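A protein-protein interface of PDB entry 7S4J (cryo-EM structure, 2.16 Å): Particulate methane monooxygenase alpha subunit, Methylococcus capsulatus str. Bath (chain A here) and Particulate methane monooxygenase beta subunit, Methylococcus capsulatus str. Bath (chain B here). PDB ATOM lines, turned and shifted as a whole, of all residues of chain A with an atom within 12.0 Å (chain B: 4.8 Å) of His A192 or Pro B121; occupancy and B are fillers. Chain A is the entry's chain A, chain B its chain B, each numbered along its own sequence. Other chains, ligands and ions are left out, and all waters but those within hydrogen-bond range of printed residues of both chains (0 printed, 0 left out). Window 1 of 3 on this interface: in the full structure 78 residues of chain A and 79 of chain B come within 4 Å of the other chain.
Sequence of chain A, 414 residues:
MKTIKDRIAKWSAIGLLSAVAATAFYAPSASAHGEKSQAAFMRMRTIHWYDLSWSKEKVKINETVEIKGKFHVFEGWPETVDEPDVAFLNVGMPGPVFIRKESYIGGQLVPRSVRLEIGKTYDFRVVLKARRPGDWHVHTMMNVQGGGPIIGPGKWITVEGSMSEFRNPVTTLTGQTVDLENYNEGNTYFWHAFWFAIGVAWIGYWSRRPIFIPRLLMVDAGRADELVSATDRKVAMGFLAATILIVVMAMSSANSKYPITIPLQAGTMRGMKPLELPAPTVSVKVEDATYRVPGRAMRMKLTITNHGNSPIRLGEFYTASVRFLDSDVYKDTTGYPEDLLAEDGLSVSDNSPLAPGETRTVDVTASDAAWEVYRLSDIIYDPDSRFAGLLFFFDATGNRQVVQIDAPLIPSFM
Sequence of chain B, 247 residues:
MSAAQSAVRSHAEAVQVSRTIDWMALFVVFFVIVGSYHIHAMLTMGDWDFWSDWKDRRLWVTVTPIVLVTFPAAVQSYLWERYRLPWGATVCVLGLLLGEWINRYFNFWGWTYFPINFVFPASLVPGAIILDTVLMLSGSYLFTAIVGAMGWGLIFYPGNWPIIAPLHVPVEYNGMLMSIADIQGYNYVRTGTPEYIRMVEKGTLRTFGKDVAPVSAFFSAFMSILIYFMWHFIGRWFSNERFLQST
Of the 22 printed residues of chain A, 7 touch a printed residue of chain B. Of the 12 printed residues of chain B, 6 touch a printed residue of chain A. Hydrophobic or aromatic side chains of chain B within 4 Å of the printed part of chain A: Trp B101, Phe B120, Pro B121 and Ile B163. Among the printed residues, no Asp or Glu carboxylate lies within 4 Å of a Lys or Arg side-chain nitrogen of the other chain.
Among the printed residues, pairs that only touch across the chains: Asn A187 with Ile B163, Thr A188 with Phe B120, Thr A188 with Ile B163, Tyr A189 with Trp B101, Trp A191 with Ile B163, His A192 with Ala B122, His A192 with Ser B123 and Trp A195 with Ser B123.
The side-chain amide oxygen (OD1) of Asn A187 is in hydrogen-bond range of the indole nitrogen (NE1) of Trp A191, at 3.1 Å. The side-chain carboxylate of Asp B49 is in hydrogen-bond range of the backbone NH of Ala B122 (2.9 Å). ND2 of Asn A187 sits at hydrogen-bond distance from OD1 of Asn A184, 3.0 Å away. The side-chain amino group (NZ) of Lys B55 sits at hydrogen-bond distance from the backbone carbonyl oxygen (O) of Phe B120 (3.2 Å). O of Asn A184 sits at hydrogen-bond distance from OG1 of Thr A188 (2.9 Å).
Printed residues of chain B within 4 Å of His A192: Trp B101, Pro B121, Ala B122 and Ser B123. Pro B121 touches just one residue of chain A: His A192 (2.8 Å). Glu B100 touches none of the printed residues of chain A. Of chain A, only Tyr A189 and His A192 come within 4 Å of Trp B101. Of chain A, only Thr A188 comes within 4 Å of Phe B120. Of chain A, only His A192 and Trp A195 come within 4 Å of Ser B123. Of the printed residues of chain B, Trp A191 touches Ile B163. Of the printed residues of chain B, Asn A187 touches Ile B163. Of the printed residues of chain B, Tyr A189 touches Trp B101 (3.7 Å). Printed residues of chain B within 4 Å of Trp A195: Ser B123 (3.5 Å). The nearest printed residue of chain B that does not touch His A192 is Leu B97 (4.02 Å). The nearest residue of chain A that does not touch Pro B121 is Thr A188 (5.7 Å). The nearest printed residue of chain B that does not touch Thr A188 is Trp B101 (4.3 Å).
O of Pro B121 lies within hydrogen-bond range of NE2 of His A192 (2.8 Å). The backbone carbonyl oxygen (O) of Ile B163 lies within hydrogen-bond range of the side-chain amide nitrogen (ND2) of Asn A184 (2.8 Å). The indole nitrogen (NE1) of Trp B101 sits at hydrogen-bond distance from a ring nitrogen (ND1) of His A192, 3.2 Å away.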
ATOM      1  N   TYR A 183     -13.805  23.333  25.475  1.00  0.00           N
ATOM      2  CA  TYR A 183     -13.441  24.305  26.495  1.00  0.00           C
ATOM      3  C   TYR A 183     -12.068  23.976  27.066  1.00  0.00           C
ATOM      4  O   TYR A 183     -11.773  22.816  27.360  1.00  0.00           O
ATOM      5  CB  TYR A 183     -14.494  24.309  27.597  1.00  0.00           C
ATOM      6  CG  TYR A 183     -14.155  25.145  28.801  1.00  0.00           C
ATOM      7  CD1 TYR A 183     -14.223  26.528  28.750  1.00  0.00           C
ATOM      8  CD2 TYR A 183     -13.776  24.550  29.993  1.00  0.00           C
ATOM      9  CE1 TYR A 183     -13.921  27.291  29.852  1.00  0.00           C
ATOM     10  CE2 TYR A 183     -13.471  25.305  31.097  1.00  0.00           C
ATOM     11  CZ  TYR A 183     -13.546  26.674  31.022  1.00  0.00           C
ATOM     12  OH  TYR A 183     -13.243  27.431  32.126  1.00  0.00           O
ATOM     13  N   ASN A 184     -11.225  25.000  27.205  1.00  0.00           N
ATOM     14  CA  ASN A 184      -9.883  24.937  27.777  1.00  0.00           C
ATOM     15  C   ASN A 184      -8.889  24.187  26.896  1.00  0.00           C
ATOM     16  O   ASN A 184      -7.722  24.047  27.282  1.00  0.00           O
ATOM     17  CB  ASN A 184      -9.890  24.314  29.183  1.00  0.00           C
ATOM     18  CG  ASN A 184      -8.661  24.663  29.982  1.00  0.00           C
ATOM     19  OD1 ASN A 184      -8.232  25.809  30.002  1.00  0.00           O
ATOM     20  ND2 ASN A 184      -8.092  23.676  30.652  1.00  0.00           N
ATOM     21  N   GLU A 185      -9.305  23.712  25.720  1.00  0.00           N
ATOM     22  CA  GLU A 185      -8.412  22.931  24.868  1.00  0.00           C
ATOM     23  C   GLU A 185      -7.213  23.758  24.417  1.00  0.00           C
ATOM     24  O   GLU A 185      -6.067  23.298  24.483  1.00  0.00           O
ATOM     25  CB  GLU A 185      -9.185  22.402  23.660  1.00  0.00           C
ATOM     26  CG  GLU A 185      -8.558  21.201  22.989  1.00  0.00           C
ATOM     27  CD  GLU A 185      -9.279  20.803  21.715  1.00  0.00           C
ATOM     28  OE1 GLU A 185     -10.508  20.593  21.763  1.00  0.00           O
ATOM     29  OE2 GLU A 185      -8.618  20.701  20.663  1.00  0.00           O
ATOM     30  N   GLY A 186      -7.464  24.984  23.958  1.00  0.00           N
ATOM     31  CA  GLY A 186      -6.378  25.827  23.490  1.00  0.00           C
ATOM     32  C   GLY A 186      -5.418  26.206  24.600  1.00  0.00           C
ATOM     33  O   GLY A 186      -4.205  26.238  24.401  1.00  0.00           O
ATOM     34  N   ASN A 187      -5.955  26.507  25.782  1.00  0.00           N
ATOM     35  CA  ASN A 187      -5.111  26.837  26.925  1.00  0.00           C
ATOM     36  C   ASN A 187      -4.226  25.659  27.318  1.00  0.00           C
ATOM     37  O   ASN A 187      -3.024  25.828  27.576  1.00  0.00           O
ATOM     38  CB  ASN A 187      -5.995  27.275  28.092  1.00  0.00           C
ATOM     39  CG  ASN A 187      -5.212  27.560  29.346  1.00  0.00           C
ATOM     40  OD1 ASN A 187      -4.410  28.486  29.391  1.00  0.00           O
ATOM     41  ND2 ASN A 187      -5.454  26.773  30.384  1.00  0.00           N
ATOM     42  N   THR A 188      -4.803  24.455  27.362  1.00  0.00           N
ATOM     43  CA  THR A 188      -4.019  23.264  27.666  1.00  0.00           C
ATOM     44  C   THR A 188      -2.914  23.053  26.641  1.00  0.00           C
ATOM     45  O   THR A 188      -1.750  22.821  27.005  1.00  0.00           O
ATOM     46  CB  THR A 188      -4.934  22.041  27.710  1.00  0.00           C
ATOM     47  OG1 THR A 188      -5.949  22.233  28.699  1.00  0.00           O
ATOM     48  CG2 THR A 188      -4.141  20.803  28.043  1.00  0.00           C
ATOM     49  N   TYR A 189      -3.264  23.149  25.356  1.00  0.00           N
ATOM     50  CA  TYR A 189      -2.280  22.993  24.294  1.00  0.00           C
ATOM     51  C   TYR A 189      -1.160  24.008  24.443  1.00  0.00           C
ATOM     52  O   TYR A 189       0.021  23.664  24.343  1.00  0.00           O
ATOM     53  CB  TYR A 189      -2.950  23.151  22.930  1.00  0.00           C
ATOM     54  CG  TYR A 189      -3.574  21.895  22.390  1.00  0.00           C
ATOM     55  CD1 TYR A 189      -2.980  20.660  22.590  1.00  0.00           C
ATOM     56  CD2 TYR A 189      -4.757  21.943  21.671  1.00  0.00           C
ATOM     57  CE1 TYR A 189      -3.549  19.512  22.096  1.00  0.00           C
ATOM     58  CE2 TYR A 189      -5.332  20.800  21.175  1.00  0.00           C
ATOM     59  CZ  TYR A 189      -4.724  19.587  21.390  1.00  0.00           C
ATOM     60  OH  TYR A 189      -5.294  18.443  20.894  1.00  0.00           O
ATOM     61  N   PHE A 190      -1.517  25.268  24.687  1.00  0.00           N
ATOM     62  CA  PHE A 190      -0.519  26.322  24.768  1.00  0.00           C
ATOM     63  C   PHE A 190       0.454  26.072  25.908  1.00  0.00           C
ATOM     64  O   PHE A 190       1.669  26.177  25.733  1.00  0.00           O
ATOM     65  CB  PHE A 190      -1.185  27.684  24.941  1.00  0.00           C
ATOM     66  CG  PHE A 190      -0.232  28.755  25.374  1.00  0.00           C
ATOM     67  CD1 PHE A 190       0.566  29.398  24.447  1.00  0.00           C
ATOM     68  CD2 PHE A 190      -0.107  29.095  26.709  1.00  0.00           C
ATOM     69  CE1 PHE A 190       1.453  30.371  24.840  1.00  0.00           C
ATOM     70  CE2 PHE A 190       0.784  30.065  27.107  1.00  0.00           C
ATOM     71  CZ  PHE A 190       1.563  30.706  26.172  1.00  0.00           C
ATOM     72  N   TRP A 191      -0.065  25.772  27.098  1.00  0.00           N
ATOM     73  CA  TRP A 191       0.830  25.621  28.241  1.00  0.00           C
ATOM     74  C   TRP A 191       1.732  24.407  28.082  1.00  0.00           C
ATOM     75  O   TRP A 191       2.938  24.476  28.368  1.00  0.00           O
ATOM     76  CB  TRP A 191       0.025  25.553  29.533  1.00  0.00           C
ATOM     77  CG  TRP A 191      -0.371  26.909  30.000  1.00  0.00           C
ATOM     78  CD1 TRP A 191      -1.635  27.391  30.134  1.00  0.00           C
ATOM     79  CD2 TRP A 191       0.507  27.974  30.375  1.00  0.00           C
ATOM     80  NE1 TRP A 191      -1.602  28.690  30.573  1.00  0.00           N
ATOM     81  CE2 TRP A 191      -0.297  29.071  30.731  1.00  0.00           C
ATOM     82  CE3 TRP A 191       1.896  28.105  30.452  1.00  0.00           C
ATOM     83  CZ2 TRP A 191       0.240  30.280  31.155  1.00  0.00           C
ATOM     84  CZ3 TRP A 191       2.425  29.305  30.869  1.00  0.00           C
ATOM     85  CH2 TRP A 191       1.601  30.377  31.214  1.00  0.00           C
ATOM     86  N   HIS A 192       1.180  23.290  27.599  1.00  0.00           N
ATOM     87  CA  HIS A 192       2.019  22.116  27.399  1.00  0.00           C
ATOM     88  C   HIS A 192       3.079  22.364  26.331  1.00  0.00           C
ATOM     89  O   HIS A 192       4.243  21.990  26.513  1.00  0.00           O
ATOM     90  CB  HIS A 192       1.156  20.908  27.055  1.00  0.00           C
ATOM     91  CG  HIS A 192       0.716  20.135  28.256  1.00  0.00           C
ATOM     92  ND1 HIS A 192       1.543  19.253  28.915  1.00  0.00           N
ATOM     93  CD2 HIS A 192      -0.457  20.125  28.930  1.00  0.00           C
ATOM     94  CE1 HIS A 192       0.895  18.723  29.934  1.00  0.00           C
ATOM     95  NE2 HIS A 192      -0.321  19.234  29.966  1.00  0.00           N
ATOM     96  N   ALA A 193       2.706  23.017  25.226  1.00  0.00           N
ATOM     97  CA  ALA A 193       3.679  23.327  24.184  1.00  0.00           C
ATOM     98  C   ALA A 193       4.749  24.283  24.689  1.00  0.00           C
ATOM     99  O   ALA A 193       5.926  24.134  24.355  1.00  0.00           O
ATOM    100  CB  ALA A 193       2.973  23.914  22.964  1.00  0.00           C
ATOM    101  N   PHE A 194       4.360  25.266  25.500  1.00  0.00           N
ATOM    102  CA  PHE A 194       5.315  26.233  26.026  1.00  0.00           C
ATOM    103  C   PHE A 194       6.353  25.555  26.910  1.00  0.00           C
ATOM    104  O   PHE A 194       7.561  25.783  26.762  1.00  0.00           O
ATOM    105  CB  PHE A 194       4.560  27.315  26.799  1.00  0.00           C
ATOM    106  CG  PHE A 194       5.440  28.240  27.578  1.00  0.00           C
ATOM    107  CD1 PHE A 194       5.996  29.352  26.976  1.00  0.00           C
ATOM    108  CD2 PHE A 194       5.707  28.004  28.915  1.00  0.00           C
ATOM    109  CE1 PHE A 194       6.805  30.207  27.690  1.00  0.00           C
ATOM    110  CE2 PHE A 194       6.516  28.853  29.632  1.00  0.00           C
ATOM    111  CZ  PHE A 194       7.066  29.958  29.019  1.00  0.00           C
ATOM    112  N   TRP A 195       5.904  24.704  27.833  1.00  0.00           N
ATOM    113  CA  TRP A 195       6.863  24.057  28.721  1.00  0.00           C
ATOM    114  C   TRP A 195       7.711  23.032  27.973  1.00  0.00           C
ATOM    115  O   TRP A 195       8.910  22.887  28.253  1.00  0.00           O
ATOM    116  CB  TRP A 195       6.139  23.433  29.909  1.00  0.00           C
ATOM    117  CG  TRP A 195       5.735  24.461  30.916  1.00  0.00           C
ATOM    118  CD1 TRP A 195       4.472  24.764  31.313  1.00  0.00           C
ATOM    119  CD2 TRP A 195       6.606  25.332  31.647  1.00  0.00           C
ATOM    120  NE1 TRP A 195       4.496  25.766  32.245  1.00  0.00           N
ATOM    121  CE2 TRP A 195       5.795  26.133  32.469  1.00  0.00           C
ATOM    122  CE3 TRP A 195       7.991  25.509  31.687  1.00  0.00           C
ATOM    123  CZ2 TRP A 195       6.323  27.095  33.323  1.00  0.00           C
ATOM    124  CZ3 TRP A 195       8.511  26.463  32.533  1.00  0.00           C
ATOM    125  CH2 TRP A 195       7.681  27.245  33.340  1.00  0.00           C
ATOM    126  N   PHE A 196       7.121  22.334  27.001  1.00  0.00           N
ATOM    127  CA  PHE A 196       7.913  21.438  26.168  1.00  0.00           C
ATOM    128  C   PHE A 196       8.989  22.203  25.409  1.00  0.00           C
ATOM    129  O   PHE A 196      10.127  21.736  25.296  1.00  0.00           O
ATOM    130  CB  PHE A 196       7.008  20.682  25.198  1.00  0.00           C
ATOM    131  CG  PHE A 196       7.594  19.396  24.706  1.00  0.00           C
ATOM    132  CD1 PHE A 196       8.442  19.380  23.614  1.00  0.00           C
ATOM    133  CD2 PHE A 196       7.302  18.202  25.335  1.00  0.00           C
ATOM    134  CE1 PHE A 196       8.983  18.201  23.159  1.00  0.00           C
ATOM    135  CE2 PHE A 196       7.843  17.018  24.883  1.00  0.00           C
ATOM    136  CZ  PHE A 196       8.684  17.019  23.794  1.00  0.00           C
ATOM    137  N   ALA A 197       8.647  23.380  24.883  1.00  0.00           N
ATOM    138  CA  ALA A 197       9.628  24.193  24.178  1.00  0.00           C
ATOM    139  C   ALA A 197      10.731  24.662  25.114  1.00  0.00           C
ATOM    140  O   ALA A 197      11.895  24.732  24.717  1.00  0.00           O
ATOM    141  CB  ALA A 197       8.945  25.386  23.512  1.00  0.00           C
ATOM    142  N   ILE A 198      10.385  24.994  26.358  1.00  0.00           N
ATOM    143  CA  ILE A 198      11.410  25.398  27.321  1.00  0.00           C
ATOM    144  C   ILE A 198      12.391  24.255  27.571  1.00  0.00           C
ATOM    145  O   ILE A 198      13.617  24.449  27.567  1.00  0.00           O
ATOM    146  CB  ILE A 198      10.754  25.878  28.629  1.00  0.00           C
ATOM    147  CG1 ILE A 198      10.080  27.234  28.425  1.00  0.00           C
ATOM    148  CG2 ILE A 198      11.779  25.958  29.744  1.00  0.00           C
ATOM    149  CD1 ILE A 198      10.998  28.298  27.902  1.00  0.00           C
ATOM    150  N   GLY A 199      11.869  23.046  27.788  1.00  0.00           N
ATOM    151  CA  GLY A 199      12.748  21.903  27.993  1.00  0.00           C
ATOM    152  C   GLY A 199      13.608  21.597  26.780  1.00  0.00           C
ATOM    153  O   GLY A 199      14.801  21.292  26.905  1.00  0.00           O
ATOM    154  N   VAL A 200      13.013  21.677  25.589  1.00  0.00           N
ATOM    155  CA  VAL A 200      13.760  21.439  24.359  1.00  0.00           C
ATOM    156  C   VAL A 200      14.839  22.497  24.181  1.00  0.00           C
ATOM    157  O   VAL A 200      15.936  22.204  23.703  1.00  0.00           O
ATOM    158  CB  VAL A 200      12.803  21.388  23.155  1.00  0.00           C
ATOM    159  CG1 VAL A 200      13.566  21.499  21.849  1.00  0.00           C
ATOM    160  CG2 VAL A 200      11.999  20.108  23.180  1.00  0.00           C
ATOM    161  N   ALA A 201      14.550  23.741  24.566  1.00  0.00           N
ATOM    162  CA  ALA A 201      15.545  24.802  24.470  1.00  0.00           C
ATOM    163  C   ALA A 201      16.724  24.531  25.391  1.00  0.00           C
ATOM    164  O   ALA A 201      17.881  24.724  25.008  1.00  0.00           O
ATOM    165  CB  ALA A 201      14.909  26.151  24.797  1.00  0.00           C
ATOM    166  N   ILE A 246       8.089  32.464  35.797  1.00  0.00           N
ATOM    167  CA  ILE A 246       6.981  32.183  34.893  1.00  0.00           C
ATOM    168  C   ILE A 246       5.906  31.382  35.606  1.00  0.00           C
ATOM    169  O   ILE A 246       4.713  31.639  35.432  1.00  0.00           O
ATOM    170  CB  ILE A 246       7.489  31.459  33.632  1.00  0.00           C
ATOM    171  CG1 ILE A 246       8.189  32.447  32.703  1.00  0.00           C
ATOM    172  CG2 ILE A 246       6.343  30.786  32.903  1.00  0.00           C
ATOM    173  CD1 ILE A 246       8.932  31.786  31.575  1.00  0.00           C
ATOM    174  N   VAL A 247       6.302  30.406  36.424  1.00  0.00           N
ATOM    175  CA  VAL A 247       5.310  29.627  37.159  1.00  0.00           C
ATOM    176  C   VAL A 247       4.515  30.530  38.094  1.00  0.00           C
ATOM    177  O   VAL A 247       3.280  30.472  38.138  1.00  0.00           O
ATOM    178  CB  VAL A 247       5.984  28.471  37.919  1.00  0.00           C
ATOM    179  CG1 VAL A 247       5.049  27.916  38.973  1.00  0.00           C
ATOM    180  CG2 VAL A 247       6.395  27.381  36.950  1.00  0.00           C
ATOM    181  N   ALA A 250       2.268  32.964  36.027  1.00  0.00           N
ATOM    182  CA  ALA A 250       1.161  32.256  35.403  1.00  0.00           C
ATOM    183  C   ALA A 250       0.118  31.844  36.430  1.00  0.00           C
ATOM    184  O   ALA A 250      -1.082  31.914  36.158  1.00  0.00           O
ATOM    185  CB  ALA A 250       1.681  31.039  34.643  1.00  0.00           C
ATOM    186  N   ASP B  49      -3.120  10.861  35.989  1.00  0.00           N
ATOM    187  CA  ASP B  49      -2.684  11.536  34.780  1.00  0.00           C
ATOM    188  C   ASP B  49      -3.674  11.406  33.634  1.00  0.00           C
ATOM    189  O   ASP B  49      -3.633  12.221  32.709  1.00  0.00           O
ATOM    190  CB  ASP B  49      -1.326  10.995  34.339  1.00  0.00           C
ATOM    191  CG  ASP B  49      -0.615  11.930  33.393  1.00  0.00           C
ATOM    192  OD1 ASP B  49      -0.280  13.056  33.807  1.00  0.00           O
ATOM    193  OD2 ASP B  49      -0.394  11.539  32.232  1.00  0.00           O
ATOM    194  N   LYS B  55      -7.391  14.932  38.641  1.00  0.00           N
ATOM    195  CA  LYS B  55      -6.340  15.878  39.036  1.00  0.00           C
ATOM    196  C   LYS B  55      -6.802  16.722  40.226  1.00  0.00           C
ATOM    197  O   LYS B  55      -7.223  17.871  40.092  1.00  0.00           O
ATOM    198  CB  LYS B  55      -5.952  16.769  37.861  1.00  0.00           C
ATOM    199  CG  LYS B  55      -5.827  16.053  36.534  1.00  0.00           C
ATOM    200  CD  LYS B  55      -4.386  15.769  36.190  1.00  0.00           C
ATOM    201  CE  LYS B  55      -4.186  15.565  34.706  1.00  0.00           C
ATOM    202  NZ  LYS B  55      -4.867  14.337  34.238  1.00  0.00           N
ATOM    203  N   LEU B  97       6.475  13.149  28.641  1.00  0.00           N
ATOM    204  CA  LEU B  97       5.436  14.002  28.080  1.00  0.00           C
ATOM    205  C   LEU B  97       5.161  13.663  26.623  1.00  0.00           C
ATOM    206  O   LEU B  97       4.006  13.658  26.193  1.00  0.00           O
ATOM    207  CB  LEU B  97       5.828  15.470  28.225  1.00  0.00           C
ATOM    208  CG  LEU B  97       5.530  16.059  29.601  1.00  0.00           C
ATOM    209  CD1 LEU B  97       6.251  17.374  29.790  1.00  0.00           C
ATOM    210  CD2 LEU B  97       4.037  16.225  29.783  1.00  0.00           C
ATOM    211  N   GLU B 100       3.252  10.299  26.541  1.00  0.00           N
ATOM    212  CA  GLU B 100       1.878  10.529  27.059  1.00  0.00           C
ATOM    213  C   GLU B 100       1.055  11.252  26.000  1.00  0.00           C
ATOM    214  O   GLU B 100      -0.025  10.749  25.676  1.00  0.00           O
ATOM    215  CB  GLU B 100       1.892  11.396  28.315  1.00  0.00           C
ATOM    216  CG  GLU B 100       2.033  10.608  29.599  1.00  0.00           C
ATOM    217  CD  GLU B 100       2.641  11.409  30.735  1.00  0.00           C
ATOM    218  OE1 GLU B 100       3.197  12.492  30.463  1.00  0.00           O
ATOM    219  OE2 GLU B 100       2.561  10.950  31.890  1.00  0.00           O
ATOM    220  N   TRP B 101       1.566  12.361  25.460  1.00  0.00           N
ATOM    221  CA  TRP B 101       0.778  13.156  24.529  1.00  0.00           C
ATOM    222  C   TRP B 101       0.483  12.396  23.248  1.00  0.00           C
ATOM    223  O   TRP B 101      -0.616  12.520  22.699  1.00  0.00           O
ATOM    224  CB  TRP B 101       1.498  14.463  24.210  1.00  0.00           C
ATOM    225  CG  TRP B 101       1.007  15.611  25.016  1.00  0.00           C
ATOM    226  CD1 TRP B 101       1.700  16.301  25.957  1.00  0.00           C
ATOM    227  CD2 TRP B 101      -0.294  16.203  24.959  1.00  0.00           C
ATOM    228  NE1 TRP B 101       0.916  17.287  26.493  1.00  0.00           N
ATOM    229  CE2 TRP B 101      -0.314  17.251  25.894  1.00  0.00           C
ATOM    230  CE3 TRP B 101      -1.441  15.951  24.205  1.00  0.00           C
ATOM    231  CZ2 TRP B 101      -1.436  18.045  26.098  1.00  0.00           C
ATOM    232  CZ3 TRP B 101      -2.551  16.738  24.408  1.00  0.00           C
ATOM    233  CH2 TRP B 101      -2.541  17.774  25.347  1.00  0.00           C
ATOM    234  N   ARG B 104      -2.319  10.143  24.202  1.00  0.00           N
ATOM    235  CA  ARG B 104      -3.552  10.887  24.438  1.00  0.00           C
ATOM    236  C   ARG B 104      -4.195  11.312  23.129  1.00  0.00           C
ATOM    237  O   ARG B 104      -5.408  11.169  22.951  1.00  0.00           O
ATOM    238  CB  ARG B 104      -3.289  12.129  25.290  1.00  0.00           C
ATOM    239  CG  ARG B 104      -2.829  11.913  26.715  1.00  0.00           C
ATOM    240  CD  ARG B 104      -3.426  10.703  27.377  1.00  0.00           C
ATOM    241  NE  ARG B 104      -2.527  10.173  28.394  1.00  0.00           N
ATOM    242  CZ  ARG B 104      -2.384  10.683  29.609  1.00  0.00           C
ATOM    243  NH1 ARG B 104      -3.058  11.753  29.994  1.00  0.00           N
ATOM    244  NH2 ARG B 104      -1.543  10.106  30.459  1.00  0.00           N
ATOM    245  N   VAL B 119      -8.575  14.505  28.718  1.00  0.00           N
ATOM    246  CA  VAL B 119      -7.544  13.489  28.916  1.00  0.00           C
ATOM    247  C   VAL B 119      -6.129  14.060  28.795  1.00  0.00           C
ATOM    248  O   VAL B 119      -5.190  13.313  28.544  1.00  0.00           O
ATOM    249  CB  VAL B 119      -7.741  12.302  27.959  1.00  0.00           C
ATOM    250  CG1 VAL B 119      -9.062  11.629  28.229  1.00  0.00           C
ATOM    251  CG2 VAL B 119      -7.646  12.759  26.517  1.00  0.00           C
ATOM    252  N   PHE B 120      -5.948  15.362  28.984  1.00  0.00           N
ATOM    253  CA  PHE B 120      -4.609  15.931  28.924  1.00  0.00           C
ATOM    254  C   PHE B 120      -3.735  15.412  30.068  1.00  0.00           C
ATOM    255  O   PHE B 120      -4.238  15.074  31.141  1.00  0.00           O
ATOM    256  CB  PHE B 120      -4.674  17.452  28.981  1.00  0.00           C
ATOM    257  CG  PHE B 120      -5.236  17.981  30.266  1.00  0.00           C
ATOM    258  CD1 PHE B 120      -6.598  18.149  30.418  1.00  0.00           C
ATOM    259  CD2 PHE B 120      -4.407  18.296  31.325  1.00  0.00           C
ATOM    260  CE1 PHE B 120      -7.118  18.626  31.594  1.00  0.00           C
ATOM    261  CE2 PHE B 120      -4.923  18.768  32.505  1.00  0.00           C
ATOM    262  CZ  PHE B 120      -6.281  18.936  32.639  1.00  0.00           C
ATOM    263  N   PRO B 121      -2.426  15.338  29.864  1.00  0.00           N
ATOM    264  CA  PRO B 121      -1.515  14.924  30.934  1.00  0.00           C
ATOM    265  C   PRO B 121      -1.084  16.113  31.789  1.00  0.00           C
ATOM    266  O   PRO B 121      -1.445  17.259  31.540  1.00  0.00           O
ATOM    267  CB  PRO B 121      -0.336  14.337  30.163  1.00  0.00           C
ATOM    268  CG  PRO B 121      -0.298  15.132  28.921  1.00  0.00           C
ATOM    269  CD  PRO B 121      -1.723  15.480  28.578  1.00  0.00           C
ATOM    270  N   ALA B 122      -0.284  15.817  32.807  1.00  0.00           N
ATOM    271  CA  ALA B 122       0.236  16.835  33.708  1.00  0.00           C
ATOM    272  C   ALA B 122       1.549  17.400  33.186  1.00  0.00           C
ATOM    273  O   ALA B 122       2.286  16.736  32.454  1.00  0.00           O
ATOM    274  CB  ALA B 122       0.441  16.263  35.109  1.00  0.00           C
ATOM    275  N   SER B 123       1.840  18.634  33.579  1.00  0.00           N
ATOM    276  CA  SER B 123       3.058  19.324  33.175  1.00  0.00           C
ATOM    277  C   SER B 123       4.156  19.086  34.207  1.00  0.00           C
ATOM    278  O   SER B 123       3.903  19.154  35.412  1.00  0.00           O
ATOM    279  CB  SER B 123       2.784  20.819  33.012  1.00  0.00           C
ATOM    280  OG  SER B 123       3.935  21.510  32.570  1.00  0.00           O
ATOM    281  N   ILE B 163      -3.376  25.377  33.751  1.00  0.00           N
ATOM    282  CA  ILE B 163      -4.111  24.456  32.890  1.00  0.00           C
ATOM    283  C   ILE B 163      -5.435  24.056  33.526  1.00  0.00           C
ATOM    284  O   ILE B 163      -6.488  24.105  32.881  1.00  0.00           O
ATOM    285  CB  ILE B 163      -3.250  23.221  32.568  1.00  0.00           C
ATOM    286  CG1 ILE B 163      -1.947  23.639  31.892  1.00  0.00           C
ATOM    287  CG2 ILE B 163      -4.017  22.251  31.690  1.00  0.00           C
ATOM    288  CD1 ILE B 163      -0.803  22.702  32.166  1.00  0.00           C
